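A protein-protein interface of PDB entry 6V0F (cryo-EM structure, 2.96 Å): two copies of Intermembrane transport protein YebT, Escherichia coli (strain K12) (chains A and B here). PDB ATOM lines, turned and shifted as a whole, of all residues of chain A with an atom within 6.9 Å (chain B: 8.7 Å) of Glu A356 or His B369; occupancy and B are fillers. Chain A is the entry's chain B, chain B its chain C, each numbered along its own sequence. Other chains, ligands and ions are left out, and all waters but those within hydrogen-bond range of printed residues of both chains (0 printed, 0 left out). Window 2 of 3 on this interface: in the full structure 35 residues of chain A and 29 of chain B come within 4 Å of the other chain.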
ATOM      1  N   THR A 353      20.570  -5.267  15.028  1.00  0.00           N
ATOM      2  CA  THR A 353      19.380  -5.927  15.545  1.00  0.00           C
ATOM      3  C   THR A 353      19.611  -6.466  16.950  1.00  0.00           C
ATOM      4  O   THR A 353      20.743  -6.680  17.381  1.00  0.00           O
ATOM      5  CB  THR A 353      18.959  -7.072  14.628  1.00  0.00           C
ATOM      6  OG1 THR A 353      20.004  -8.047  14.579  1.00  0.00           O
ATOM      7  CG2 THR A 353      18.705  -6.560  13.230  1.00  0.00           C
ATOM      8  N   ALA A 354      18.508  -6.706  17.654  1.00  0.00           N
ATOM      9  CA  ALA A 354      18.541  -7.195  19.024  1.00  0.00           C
ATOM     10  C   ALA A 354      17.194  -7.817  19.332  1.00  0.00           C
ATOM     11  O   ALA A 354      16.188  -7.392  18.762  1.00  0.00           O
ATOM     12  CB  ALA A 354      18.839  -6.059  20.012  1.00  0.00           C
ATOM     13  N   PRO A 355      17.133  -8.828  20.200  1.00  0.00           N
ATOM     14  CA  PRO A 355      15.836  -9.418  20.545  1.00  0.00           C
ATOM     15  C   PRO A 355      15.098  -8.670  21.639  1.00  0.00           C
ATOM     16  O   PRO A 355      13.991  -9.074  22.003  1.00  0.00           O
ATOM     17  CB  PRO A 355      16.222 -10.816  21.026  1.00  0.00           C
ATOM     18  CG  PRO A 355      17.552 -10.619  21.621  1.00  0.00           C
ATOM     19  CD  PRO A 355      18.246  -9.595  20.781  1.00  0.00           C
ATOM     20  N   GLU A 356      15.683  -7.597  22.156  1.00  0.00           N
ATOM     21  CA  GLU A 356      15.119  -6.827  23.250  1.00  0.00           C
ATOM     22  C   GLU A 356      15.808  -5.474  23.215  1.00  0.00           C
ATOM     23  O   GLU A 356      16.927  -5.360  22.714  1.00  0.00           O
ATOM     24  CB  GLU A 356      15.341  -7.552  24.582  1.00  0.00           C
ATOM     25  CG  GLU A 356      14.604  -7.009  25.783  1.00  0.00           C
ATOM     26  CD  GLU A 356      14.834  -7.857  27.014  1.00  0.00           C
ATOM     27  OE1 GLU A 356      15.568  -8.859  26.916  1.00  0.00           O
ATOM     28  OE2 GLU A 356      14.283  -7.524  28.081  1.00  0.00           O
ATOM     29  N   SER A 357      15.129  -4.446  23.723  1.00  0.00           N
ATOM     30  CA  SER A 357      15.714  -3.111  23.701  1.00  0.00           C
ATOM     31  C   SER A 357      16.885  -2.982  24.655  1.00  0.00           C
ATOM     32  O   SER A 357      17.749  -2.125  24.443  1.00  0.00           O
ATOM     33  CB  SER A 357      14.670  -2.060  24.040  1.00  0.00           C
ATOM     34  OG  SER A 357      15.245  -0.775  24.089  1.00  0.00           O
ATOM     35  N   TYR A 358      16.905  -3.795  25.715  1.00  0.00           N
ATOM     36  CA  TYR A 358      17.898  -3.760  26.794  1.00  0.00           C
ATOM     37  C   TYR A 358      17.961  -2.391  27.459  1.00  0.00           C
ATOM     38  O   TYR A 358      19.004  -1.990  27.969  1.00  0.00           O
ATOM     39  CB  TYR A 358      19.295  -4.174  26.319  1.00  0.00           C
ATOM     40  CG  TYR A 358      19.405  -5.607  25.870  1.00  0.00           C
ATOM     41  CD1 TYR A 358      19.429  -6.642  26.785  1.00  0.00           C
ATOM     42  CD2 TYR A 358      19.530  -5.917  24.529  1.00  0.00           C
ATOM     43  CE1 TYR A 358      19.539  -7.950  26.370  1.00  0.00           C
ATOM     44  CE2 TYR A 358      19.641  -7.218  24.107  1.00  0.00           C
ATOM     45  CZ  TYR A 358      19.646  -8.229  25.031  1.00  0.00           C
ATOM     46  OH  TYR A 358      19.761  -9.526  24.606  1.00  0.00           O
ATOM     47  N   GLY A 359      16.847  -1.665  27.466  1.00  0.00           N
ATOM     48  CA  GLY A 359      16.817  -0.345  28.054  1.00  0.00           C
ATOM     49  C   GLY A 359      17.584   0.717  27.303  1.00  0.00           C
ATOM     50  O   GLY A 359      17.974   1.719  27.903  1.00  0.00           O
ATOM     51  N   ILE A 360      17.817   0.532  26.010  1.00  0.00           N
ATOM     52  CA  ILE A 360      18.575   1.484  25.207  1.00  0.00           C
ATOM     53  C   ILE A 360      17.588   2.419  24.527  1.00  0.00           C
ATOM     54  O   ILE A 360      16.800   2.001  23.675  1.00  0.00           O
ATOM     55  CB  ILE A 360      19.463   0.774  24.180  1.00  0.00           C
ATOM     56  CG1 ILE A 360      20.514  -0.066  24.886  1.00  0.00           C
ATOM     57  CG2 ILE A 360      20.117   1.767  23.266  1.00  0.00           C
ATOM     58  CD1 ILE A 360      21.286  -0.945  23.965  1.00  0.00           C
ATOM     59  N   ARG A 379      15.338   3.912  17.380  1.00  0.00           N
ATOM     60  CA  ARG A 379      15.005   2.558  17.787  1.00  0.00           C
ATOM     61  C   ARG A 379      13.649   2.201  17.208  1.00  0.00           C
ATOM     62  O   ARG A 379      12.652   2.861  17.508  1.00  0.00           O
ATOM     63  CB  ARG A 379      14.974   2.466  19.304  1.00  0.00           C
ATOM     64  CG  ARG A 379      14.588   1.133  19.826  1.00  0.00           C
ATOM     65  CD  ARG A 379      14.539   1.171  21.327  1.00  0.00           C
ATOM     66  NE  ARG A 379      13.528   2.101  21.798  1.00  0.00           N
ATOM     67  CZ  ARG A 379      13.392   2.458  23.066  1.00  0.00           C
ATOM     68  NH1 ARG A 379      14.202   1.955  23.981  1.00  0.00           N
ATOM     69  NH2 ARG A 379      12.444   3.308  23.418  1.00  0.00           N
ATOM     70  N   LEU A 381      10.754  -0.816  16.598  1.00  0.00           N
ATOM     71  CA  LEU A 381      10.247  -2.087  17.087  1.00  0.00           C
ATOM     72  C   LEU A 381       9.597  -2.848  15.943  1.00  0.00           C
ATOM     73  O   LEU A 381       8.679  -2.339  15.295  1.00  0.00           O
ATOM     74  CB  LEU A 381       9.276  -1.837  18.241  1.00  0.00           C
ATOM     75  CG  LEU A 381       8.470  -2.884  19.021  1.00  0.00           C
ATOM     76  CD1 LEU A 381       7.274  -3.452  18.301  1.00  0.00           C
ATOM     77  CD2 LEU A 381       9.396  -3.999  19.447  1.00  0.00           C
ATOM     78  N   THR A 382      10.057  -4.067  15.709  1.00  0.00           N
ATOM     79  CA  THR A 382       9.551  -4.937  14.661  1.00  0.00           C
ATOM     80  C   THR A 382       9.008  -6.216  15.286  1.00  0.00           C
ATOM     81  O   THR A 382       9.063  -6.412  16.500  1.00  0.00           O
ATOM     82  CB  THR A 382      10.636  -5.261  13.634  1.00  0.00           C
ATOM     83  OG1 THR A 382      11.733  -5.906  14.289  1.00  0.00           O
ATOM     84  CG2 THR A 382      11.124  -3.999  12.953  1.00  0.00           C
ATOM     85  N   SER A 383       8.481  -7.096  14.438  1.00  0.00           N
ATOM     86  CA  SER A 383       7.976  -8.375  14.917  1.00  0.00           C
ATOM     87  C   SER A 383       9.097  -9.359  15.214  1.00  0.00           C
ATOM     88  O   SER A 383       8.940 -10.223  16.082  1.00  0.00           O
ATOM     89  CB  SER A 383       7.018  -8.978  13.897  1.00  0.00           C
ATOM     90  OG  SER A 383       7.707  -9.299  12.703  1.00  0.00           O
ATOM     91  N   LYS A 384      10.226  -9.252  14.510  1.00  0.00           N
ATOM     92  CA  LYS A 384      11.366 -10.112  14.815  1.00  0.00           C
ATOM     93  C   LYS A 384      12.069  -9.672  16.091  1.00  0.00           C
ATOM     94  O   LYS A 384      12.608 -10.509  16.821  1.00  0.00           O
ATOM     95  CB  LYS A 384      12.366 -10.114  13.657  1.00  0.00           C
ATOM     96  CG  LYS A 384      12.106 -11.142  12.563  1.00  0.00           C
ATOM     97  CD  LYS A 384      10.969 -10.740  11.639  1.00  0.00           C
ATOM     98  CE  LYS A 384      11.355  -9.542  10.794  1.00  0.00           C
ATOM     99  NZ  LYS A 384      10.267  -9.167   9.851  1.00  0.00           N
ATOM    100  N   GLY A 385      12.087  -8.375  16.364  1.00  0.00           N
ATOM    101  CA  GLY A 385      12.739  -7.878  17.562  1.00  0.00           C
ATOM    102  C   GLY A 385      12.788  -6.370  17.544  1.00  0.00           C
ATOM    103  O   GLY A 385      11.889  -5.710  17.018  1.00  0.00           O
ATOM    104  N   VAL A 386      13.853  -5.838  18.124  1.00  0.00           N
ATOM    105  CA  VAL A 386      14.110  -4.409  18.160  1.00  0.00           C
ATOM    106  C   VAL A 386      15.320  -4.134  17.290  1.00  0.00           C
ATOM    107  O   VAL A 386      16.397  -4.691  17.526  1.00  0.00           O
ATOM    108  CB  VAL A 386      14.338  -3.924  19.592  1.00  0.00           C
ATOM    109  CG1 VAL A 386      14.759  -2.507  19.582  1.00  0.00           C
ATOM    110  CG2 VAL A 386      13.074  -4.070  20.380  1.00  0.00           C
ATOM    111  N   PHE A 388      17.894  -1.289  15.989  1.00  0.00           N
ATOM    112  CA  PHE A 388      18.450   0.028  16.219  1.00  0.00           C
ATOM    113  C   PHE A 388      19.092   0.527  14.938  1.00  0.00           C
ATOM    114  O   PHE A 388      19.508  -0.257  14.080  1.00  0.00           O
ATOM    115  CB  PHE A 388      19.516  -0.023  17.307  1.00  0.00           C
ATOM    116  CG  PHE A 388      18.998  -0.384  18.647  1.00  0.00           C
ATOM    117  CD1 PHE A 388      18.460   0.573  19.473  1.00  0.00           C
ATOM    118  CD2 PHE A 388      19.055  -1.690  19.081  1.00  0.00           C
ATOM    119  CE1 PHE A 388      17.993   0.233  20.706  1.00  0.00           C
ATOM    120  CE2 PHE A 388      18.590  -2.035  20.306  1.00  0.00           C
ATOM    121  CZ  PHE A 388      18.056  -1.075  21.121  1.00  0.00           C
ATOM    122  N   VAL A 408      25.950  -4.544  25.215  1.00  0.00           N
ATOM    123  CA  VAL A 408      25.110  -3.564  25.897  1.00  0.00           C
ATOM    124  C   VAL A 408      25.821  -3.044  27.142  1.00  0.00           C
ATOM    125  O   VAL A 408      26.391  -3.821  27.916  1.00  0.00           O
ATOM    126  CB  VAL A 408      23.756  -4.199  26.238  1.00  0.00           C
ATOM    127  CG1 VAL A 408      22.883  -3.262  27.010  1.00  0.00           C
ATOM    128  CG2 VAL A 408      23.054  -4.604  24.981  1.00  0.00           C
ATOM    129  N   ARG A 411      22.854  -2.340  31.280  1.00  0.00           N
ATOM    130  CA  ARG A 411      22.490  -3.183  32.406  1.00  0.00           C
ATOM    131  C   ARG A 411      23.706  -3.516  33.255  1.00  0.00           C
ATOM    132  O   ARG A 411      24.793  -3.767  32.728  1.00  0.00           O
ATOM    133  CB  ARG A 411      21.856  -4.470  31.912  1.00  0.00           C
ATOM    134  CG  ARG A 411      20.520  -4.287  31.250  1.00  0.00           C
ATOM    135  CD  ARG A 411      19.958  -5.631  30.856  1.00  0.00           C
ATOM    136  NE  ARG A 411      20.760  -6.245  29.801  1.00  0.00           N
ATOM    137  CZ  ARG A 411      21.484  -7.348  29.953  1.00  0.00           C
ATOM    138  NH1 ARG A 411      22.186  -7.833  28.937  1.00  0.00           N
ATOM    139  NH2 ARG A 411      21.509  -7.966  31.124  1.00  0.00           N
ATOM    140  N   LEU A 452      23.358  -7.379  18.438  1.00  0.00           N
ATOM    141  CA  LEU A 452      23.660  -6.709  19.691  1.00  0.00           C
ATOM    142  C   LEU A 452      23.672  -7.776  20.772  1.00  0.00           C
ATOM    143  O   LEU A 452      22.639  -8.385  21.061  1.00  0.00           O
ATOM    144  CB  LEU A 452      22.634  -5.624  19.985  1.00  0.00           C
ATOM    145  CG  LEU A 452      22.842  -4.837  21.266  1.00  0.00           C
ATOM    146  CD1 LEU A 452      24.169  -4.145  21.230  1.00  0.00           C
ATOM    147  CD2 LEU A 452      21.739  -3.837  21.444  1.00  0.00           C
ATOM    148  N   LEU B 366       3.606   1.024  29.504  1.00  0.00           N
ATOM    149  CA  LEU B 366       3.406  -0.399  29.277  1.00  0.00           C
ATOM    150  C   LEU B 366       4.341  -0.860  28.168  1.00  0.00           C
ATOM    151  O   LEU B 366       4.323  -0.310  27.064  1.00  0.00           O
ATOM    152  CB  LEU B 366       1.944  -0.660  28.938  1.00  0.00           C
ATOM    153  CG  LEU B 366       1.451  -2.070  28.699  1.00  0.00           C
ATOM    154  CD1 LEU B 366       0.116  -2.222  29.333  1.00  0.00           C
ATOM    155  CD2 LEU B 366       1.296  -2.241  27.263  1.00  0.00           C
ATOM    156  N   ILE B 367       5.127  -1.892  28.459  1.00  0.00           N
ATOM    157  CA  ILE B 367       6.416  -2.129  27.819  1.00  0.00           C
ATOM    158  C   ILE B 367       6.425  -3.487  27.137  1.00  0.00           C
ATOM    159  O   ILE B 367       6.147  -4.504  27.773  1.00  0.00           O
ATOM    160  CB  ILE B 367       7.552  -2.038  28.849  1.00  0.00           C
ATOM    161  CG1 ILE B 367       7.663  -0.616  29.378  1.00  0.00           C
ATOM    162  CG2 ILE B 367       8.848  -2.475  28.255  1.00  0.00           C
ATOM    163  CD1 ILE B 367       8.563  -0.492  30.569  1.00  0.00           C
ATOM    164  N   LEU B 368       6.766  -3.507  25.855  1.00  0.00           N
ATOM    165  CA  LEU B 368       7.075  -4.738  25.142  1.00  0.00           C
ATOM    166  C   LEU B 368       8.510  -4.677  24.663  1.00  0.00           C
ATOM    167  O   LEU B 368       8.906  -3.696  24.032  1.00  0.00           O
ATOM    168  CB  LEU B 368       6.134  -4.975  23.960  1.00  0.00           C
ATOM    169  CG  LEU B 368       6.273  -6.329  23.254  1.00  0.00           C
ATOM    170  CD1 LEU B 368       4.959  -6.752  22.802  1.00  0.00           C
ATOM    171  CD2 LEU B 368       7.131  -6.266  22.011  1.00  0.00           C
ATOM    172  N   HIS B 369       9.291  -5.702  25.019  1.00  0.00           N
ATOM    173  CA  HIS B 369      10.676  -5.891  24.575  1.00  0.00           C
ATOM    174  C   HIS B 369      11.573  -4.712  24.909  1.00  0.00           C
ATOM    175  O   HIS B 369      12.543  -4.456  24.205  1.00  0.00           O
ATOM    176  CB  HIS B 369      10.756  -6.182  23.076  1.00  0.00           C
ATOM    177  CG  HIS B 369      10.317  -7.559  22.705  1.00  0.00           C
ATOM    178  ND1 HIS B 369      10.133  -7.952  21.398  1.00  0.00           N
ATOM    179  CD2 HIS B 369      10.037  -8.642  23.465  1.00  0.00           C
ATOM    180  CE1 HIS B 369       9.752  -9.216  21.370  1.00  0.00           C
ATOM    181  NE2 HIS B 369       9.683  -9.657  22.611  1.00  0.00           N
ATOM    182  N   GLY B 370      11.250  -3.984  25.965  1.00  0.00           N
ATOM    183  CA  GLY B 370      12.006  -2.836  26.386  1.00  0.00           C
ATOM    184  C   GLY B 370      11.475  -1.506  25.891  1.00  0.00           C
ATOM    185  O   GLY B 370      11.778  -0.478  26.503  1.00  0.00           O
ATOM    186  N   VAL B 371      10.687  -1.493  24.817  1.00  0.00           N
ATOM    187  CA  VAL B 371      10.155  -0.252  24.263  1.00  0.00           C
ATOM    188  C   VAL B 371       8.697  -0.096  24.679  1.00  0.00           C
ATOM    189  O   VAL B 371       7.955  -1.078  24.785  1.00  0.00           O
ATOM    190  CB  VAL B 371      10.353  -0.199  22.733  1.00  0.00           C
ATOM    191  CG1 VAL B 371       9.578  -1.238  22.038  1.00  0.00           C
ATOM    192  CG2 VAL B 371      10.021   1.167  22.163  1.00  0.00           C
ATOM    193  N   GLN B 372       8.304   1.133  24.997  1.00  0.00           N
ATOM    194  CA  GLN B 372       6.936   1.418  25.406  1.00  0.00           C
ATOM    195  C   GLN B 372       5.988   1.319  24.224  1.00  0.00           C
ATOM    196  O   GLN B 372       6.119   2.072  23.256  1.00  0.00           O
ATOM    197  CB  GLN B 372       6.856   2.809  26.018  1.00  0.00           C
ATOM    198  CG  GLN B 372       5.464   3.192  26.431  1.00  0.00           C
ATOM    199  CD  GLN B 372       5.403   4.561  27.047  1.00  0.00           C
ATOM    200  OE1 GLN B 372       6.415   5.243  27.160  1.00  0.00           O
ATOM    201  NE2 GLN B 372       4.212   4.985  27.437  1.00  0.00           N
ATOM    202  N   VAL B 373       5.018   0.413  24.302  1.00  0.00           N
ATOM    203  CA  VAL B 373       4.031   0.263  23.239  1.00  0.00           C
ATOM    204  C   VAL B 373       2.671   0.787  23.629  1.00  0.00           C
ATOM    205  O   VAL B 373       1.804   0.923  22.753  1.00  0.00           O
ATOM    206  CB  VAL B 373       3.899  -1.200  22.777  1.00  0.00           C
ATOM    207  CG1 VAL B 373       5.196  -1.702  22.201  1.00  0.00           C
ATOM    208  CG2 VAL B 373       3.434  -2.059  23.911  1.00  0.00           C
ATOM    209  N   HIS B 396       1.824  -2.163  18.636  1.00  0.00           N
ATOM    210  CA  HIS B 396       1.416  -3.404  19.289  1.00  0.00           C
ATOM    211  C   HIS B 396       0.027  -3.905  18.909  1.00  0.00           C
ATOM    212  O   HIS B 396      -0.260  -5.074  19.190  1.00  0.00           O
ATOM    213  CB  HIS B 396       1.555  -3.231  20.813  1.00  0.00           C
ATOM    214  CG  HIS B 396       1.298  -4.476  21.614  1.00  0.00           C
ATOM    215  ND1 HIS B 396       2.050  -5.624  21.488  1.00  0.00           N
ATOM    216  CD2 HIS B 396       0.403  -4.725  22.599  1.00  0.00           C
ATOM    217  CE1 HIS B 396       1.588  -6.543  22.318  1.00  0.00           C
ATOM    218  NE2 HIS B 396       0.620  -6.007  23.034  1.00  0.00           N
ATOM    219  N   LEU B 399       1.076  -6.485  16.491  1.00  0.00           N
ATOM    220  CA  LEU B 399       1.816  -7.457  17.316  1.00  0.00           C
ATOM    221  C   LEU B 399       1.050  -8.513  18.121  1.00  0.00           C
ATOM    222  O   LEU B 399       1.545  -9.640  18.236  1.00  0.00           O
ATOM    223  CB  LEU B 399       2.757  -6.760  18.287  1.00  0.00           C
ATOM    224  CG  LEU B 399       4.179  -6.487  17.815  1.00  0.00           C
ATOM    225  CD1 LEU B 399       4.370  -5.503  16.690  1.00  0.00           C
ATOM    226  CD2 LEU B 399       4.948  -6.107  19.032  1.00  0.00           C
ATOM    227  N   ASN B 409       6.314  -5.060  36.110  1.00  0.00           N
ATOM    228  CA  ASN B 409       7.664  -4.505  36.185  1.00  0.00           C
ATOM    229  C   ASN B 409       7.843  -3.514  37.323  1.00  0.00           C
ATOM    230  O   ASN B 409       8.856  -2.810  37.354  1.00  0.00           O
ATOM    231  CB  ASN B 409       8.063  -3.770  34.905  1.00  0.00           C
ATOM    232  CG  ASN B 409       8.510  -4.680  33.807  1.00  0.00           C
ATOM    233  OD1 ASN B 409       9.117  -5.719  34.040  1.00  0.00           O
ATOM    234  ND2 ASN B 409       8.320  -4.228  32.581  1.00  0.00           N
ATOM    235  N   GLU B 430      13.856   0.545  34.849  1.00  0.00           N
ATOM    236  CA  GLU B 430      12.548  -0.078  34.713  1.00  0.00           C
ATOM    237  C   GLU B 430      11.677   0.251  35.917  1.00  0.00           C
ATOM    238  O   GLU B 430      10.524   0.652  35.764  1.00  0.00           O
ATOM    239  CB  GLU B 430      12.702  -1.588  34.538  1.00  0.00           C
ATOM    240  CG  GLU B 430      13.436  -1.997  33.273  1.00  0.00           C
ATOM    241  CD  GLU B 430      12.765  -1.501  32.015  1.00  0.00           C
ATOM    242  OE1 GLU B 430      11.518  -1.524  31.948  1.00  0.00           O
ATOM    243  OE2 GLU B 430      13.486  -1.078  31.089  1.00  0.00           O
ATOM    244  N   ILE B 436       3.805  -2.459  33.093  1.00  0.00           N
ATOM    245  CA  ILE B 436       3.432  -3.826  32.755  1.00  0.00           C
ATOM    246  C   ILE B 436       4.239  -4.274  31.544  1.00  0.00           C
ATOM    247  O   ILE B 436       4.400  -3.513  30.585  1.00  0.00           O
ATOM    248  CB  ILE B 436       1.921  -3.940  32.502  1.00  0.00           C
ATOM    249  CG1 ILE B 436       1.156  -3.534  33.748  1.00  0.00           C
ATOM    250  CG2 ILE B 436       1.526  -5.342  32.177  1.00  0.00           C
ATOM    251  CD1 ILE B 436      -0.309  -3.384  33.513  1.00  0.00           C
ATOM    252  N   ARG B 437       4.774  -5.485  31.609  1.00  0.00           N
ATOM    253  CA  ARG B 437       5.569  -6.103  30.562  1.00  0.00           C
ATOM    254  C   ARG B 437       4.729  -7.121  29.806  1.00  0.00           C
ATOM    255  O   ARG B 437       3.907  -7.817  30.401  1.00  0.00           O
ATOM    256  CB  ARG B 437       6.785  -6.792  31.174  1.00  0.00           C
ATOM    257  CG  ARG B 437       7.807  -7.330  30.211  1.00  0.00           C
ATOM    258  CD  ARG B 437       9.010  -7.830  30.985  1.00  0.00           C
ATOM    259  NE  ARG B 437      10.074  -8.280  30.102  1.00  0.00           N
ATOM    260  CZ  ARG B 437      10.216  -9.534  29.700  1.00  0.00           C
ATOM    261  NH1 ARG B 437       9.368 -10.454  30.119  1.00  0.00           N
ATOM    262  NH2 ARG B 437      11.210  -9.866  28.892  1.00  0.00           N
ATOM    263  N   ILE B 438       4.918  -7.181  28.490  1.00  0.00           N
ATOM    264  CA  ILE B 438       4.156  -8.067  27.615  1.00  0.00           C
ATOM    265  C   ILE B 438       5.025  -9.246  27.204  1.00  0.00           C
ATOM    266  O   ILE B 438       6.187  -9.070  26.822  1.00  0.00           O
ATOM    267  CB  ILE B 438       3.649  -7.319  26.377  1.00  0.00           C
ATOM    268  CG1 ILE B 438       2.833  -6.117  26.796  1.00  0.00           C
ATOM    269  CG2 ILE B 438       2.764  -8.201  25.538  1.00  0.00           C
ATOM    270  CD1 ILE B 438       2.521  -5.259  25.658  1.00  0.00           C
ATOM    271  N   LEU B 439       4.465 -10.444  27.282  1.00  0.00           N
ATOM    272  CA  LEU B 439       5.038 -11.646  26.694  1.00  0.00           C
ATOM    273  C   LEU B 439       4.199 -12.058  25.494  1.00  0.00           C
ATOM    274  O   LEU B 439       3.154 -12.703  25.664  1.00  0.00           O
ATOM    275  CB  LEU B 439       5.086 -12.770  27.725  1.00  0.00           C
ATOM    276  CG  LEU B 439       6.058 -12.532  28.865  1.00  0.00           C
ATOM    277  CD1 LEU B 439       5.889 -13.611  29.897  1.00  0.00           C
ATOM    278  CD2 LEU B 439       7.449 -12.551  28.307  1.00  0.00           C
ATOM    279  N   PRO B 440       4.586 -11.690  24.276  1.00  0.00           N
ATOM    280  CA  PRO B 440       3.714 -11.915  23.121  1.00  0.00           C
ATOM    281  C   PRO B 440       3.663 -13.376  22.716  1.00  0.00           C
ATOM    282  O   PRO B 440       4.641 -14.116  22.841  1.00  0.00           O
ATOM    283  CB  PRO B 440       4.363 -11.067  22.025  1.00  0.00           C
ATOM    284  CG  PRO B 440       5.787 -11.014  22.407  1.00  0.00           C
ATOM    285  CD  PRO B 440       5.822 -10.988  23.901  1.00  0.00           C
ATOM    286  N   GLY B 441       2.493 -13.794  22.235  1.00  0.00           N
ATOM    287  CA  GLY B 441       2.272 -15.146  21.782  1.00  0.00           C
ATOM    288  C   GLY B 441       2.093 -15.223  20.274  1.00  0.00           C
ATOM    289  O   GLY B 441       2.189 -14.239  19.546  1.00  0.00           O
ATOM    290  N   LEU B 456       7.679 -13.135  36.366  1.00  0.00           N
ATOM    291  CA  LEU B 456       7.834 -13.796  35.080  1.00  0.00           C
ATOM    292  C   LEU B 456       7.638 -15.301  35.202  1.00  0.00           C
ATOM    293  O   LEU B 456       7.031 -15.921  34.321  1.00  0.00           O
ATOM    294  CB  LEU B 456       9.201 -13.450  34.493  1.00  0.00           C
ATOM    295  CG  LEU B 456       9.504 -13.731  33.022  1.00  0.00           C
ATOM    296  CD1 LEU B 456      10.437 -12.659  32.516  1.00  0.00           C
ATOM    297  CD2 LEU B 456      10.162 -15.075  32.823  1.00  0.00           C
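The side-chain carboxylate of Glu A356 is in salt-bridge range of the guanidinium group of Arg B437, at 3.9 Å. N of Ser A357 lies within hydrogen-bond range of O of His B369.
O of Ile A360 lies within hydrogen-bond range of NH1 of Arg A379 (2.6 Å). NH1 of Arg A379 sits at hydrogen-bond distance from OG of Ser A357 (2.9 Å). The backbone carbonyl oxygen of Ile A360 sits at hydrogen-bond distance from the side-chain hydroxyl of Ser A357 (3.2 Å). N of Val A386 sits at hydrogen-bond distance from O of Ala A354, 2.9 Å away.
O of His B369 touches C of Glu A356, at 3.6 Å. Ser A357 touches Gly B370. Arg A379 touches Val B371. Val B371 touches Leu A381 (CG1 to CG, 3.6 Å). Leu A381 touches Leu B399. His B369 touches Val A386.
Of chain B, only His B369 and Arg B437 come within 4 Å of Glu A356. Of chain A, only Glu A356, Ser A357 and Val A386 come within 4 Å of His B369. Of the printed residues of chain B, Ser A357 touches His B369 (2.6 Å) and Gly B370 (3.6 Å). Printed residues of chain A within 4 Å of Leu B399: Leu A381. Of the printed residues of chain B, Leu A381 touches Val B371 (3.6 Å) and Leu B399 (3.6 Å). Printed residues of chain A within 4 Å of Gly B370: Ser A357 (3.6 Å). Of the printed residues of chain B, Val A386 touches His B369. Of the printed residues of chain A, Arg B437 touches Glu A356 (3.9 Å). Leu B366 touches none of the printed residues of chain A. The nearest printed residue of chain A that does not touch Val B371 is Ser A357 (4.1 Å).
Hydrophobic or aromatic side chains of chain B that line the printed part of chain A: Val B371 and Leu B399.
No position is printed for both chains. Of the 8 pairs that touch across the chains among the printed residues, none has its exchanged pair printed and touching as well.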
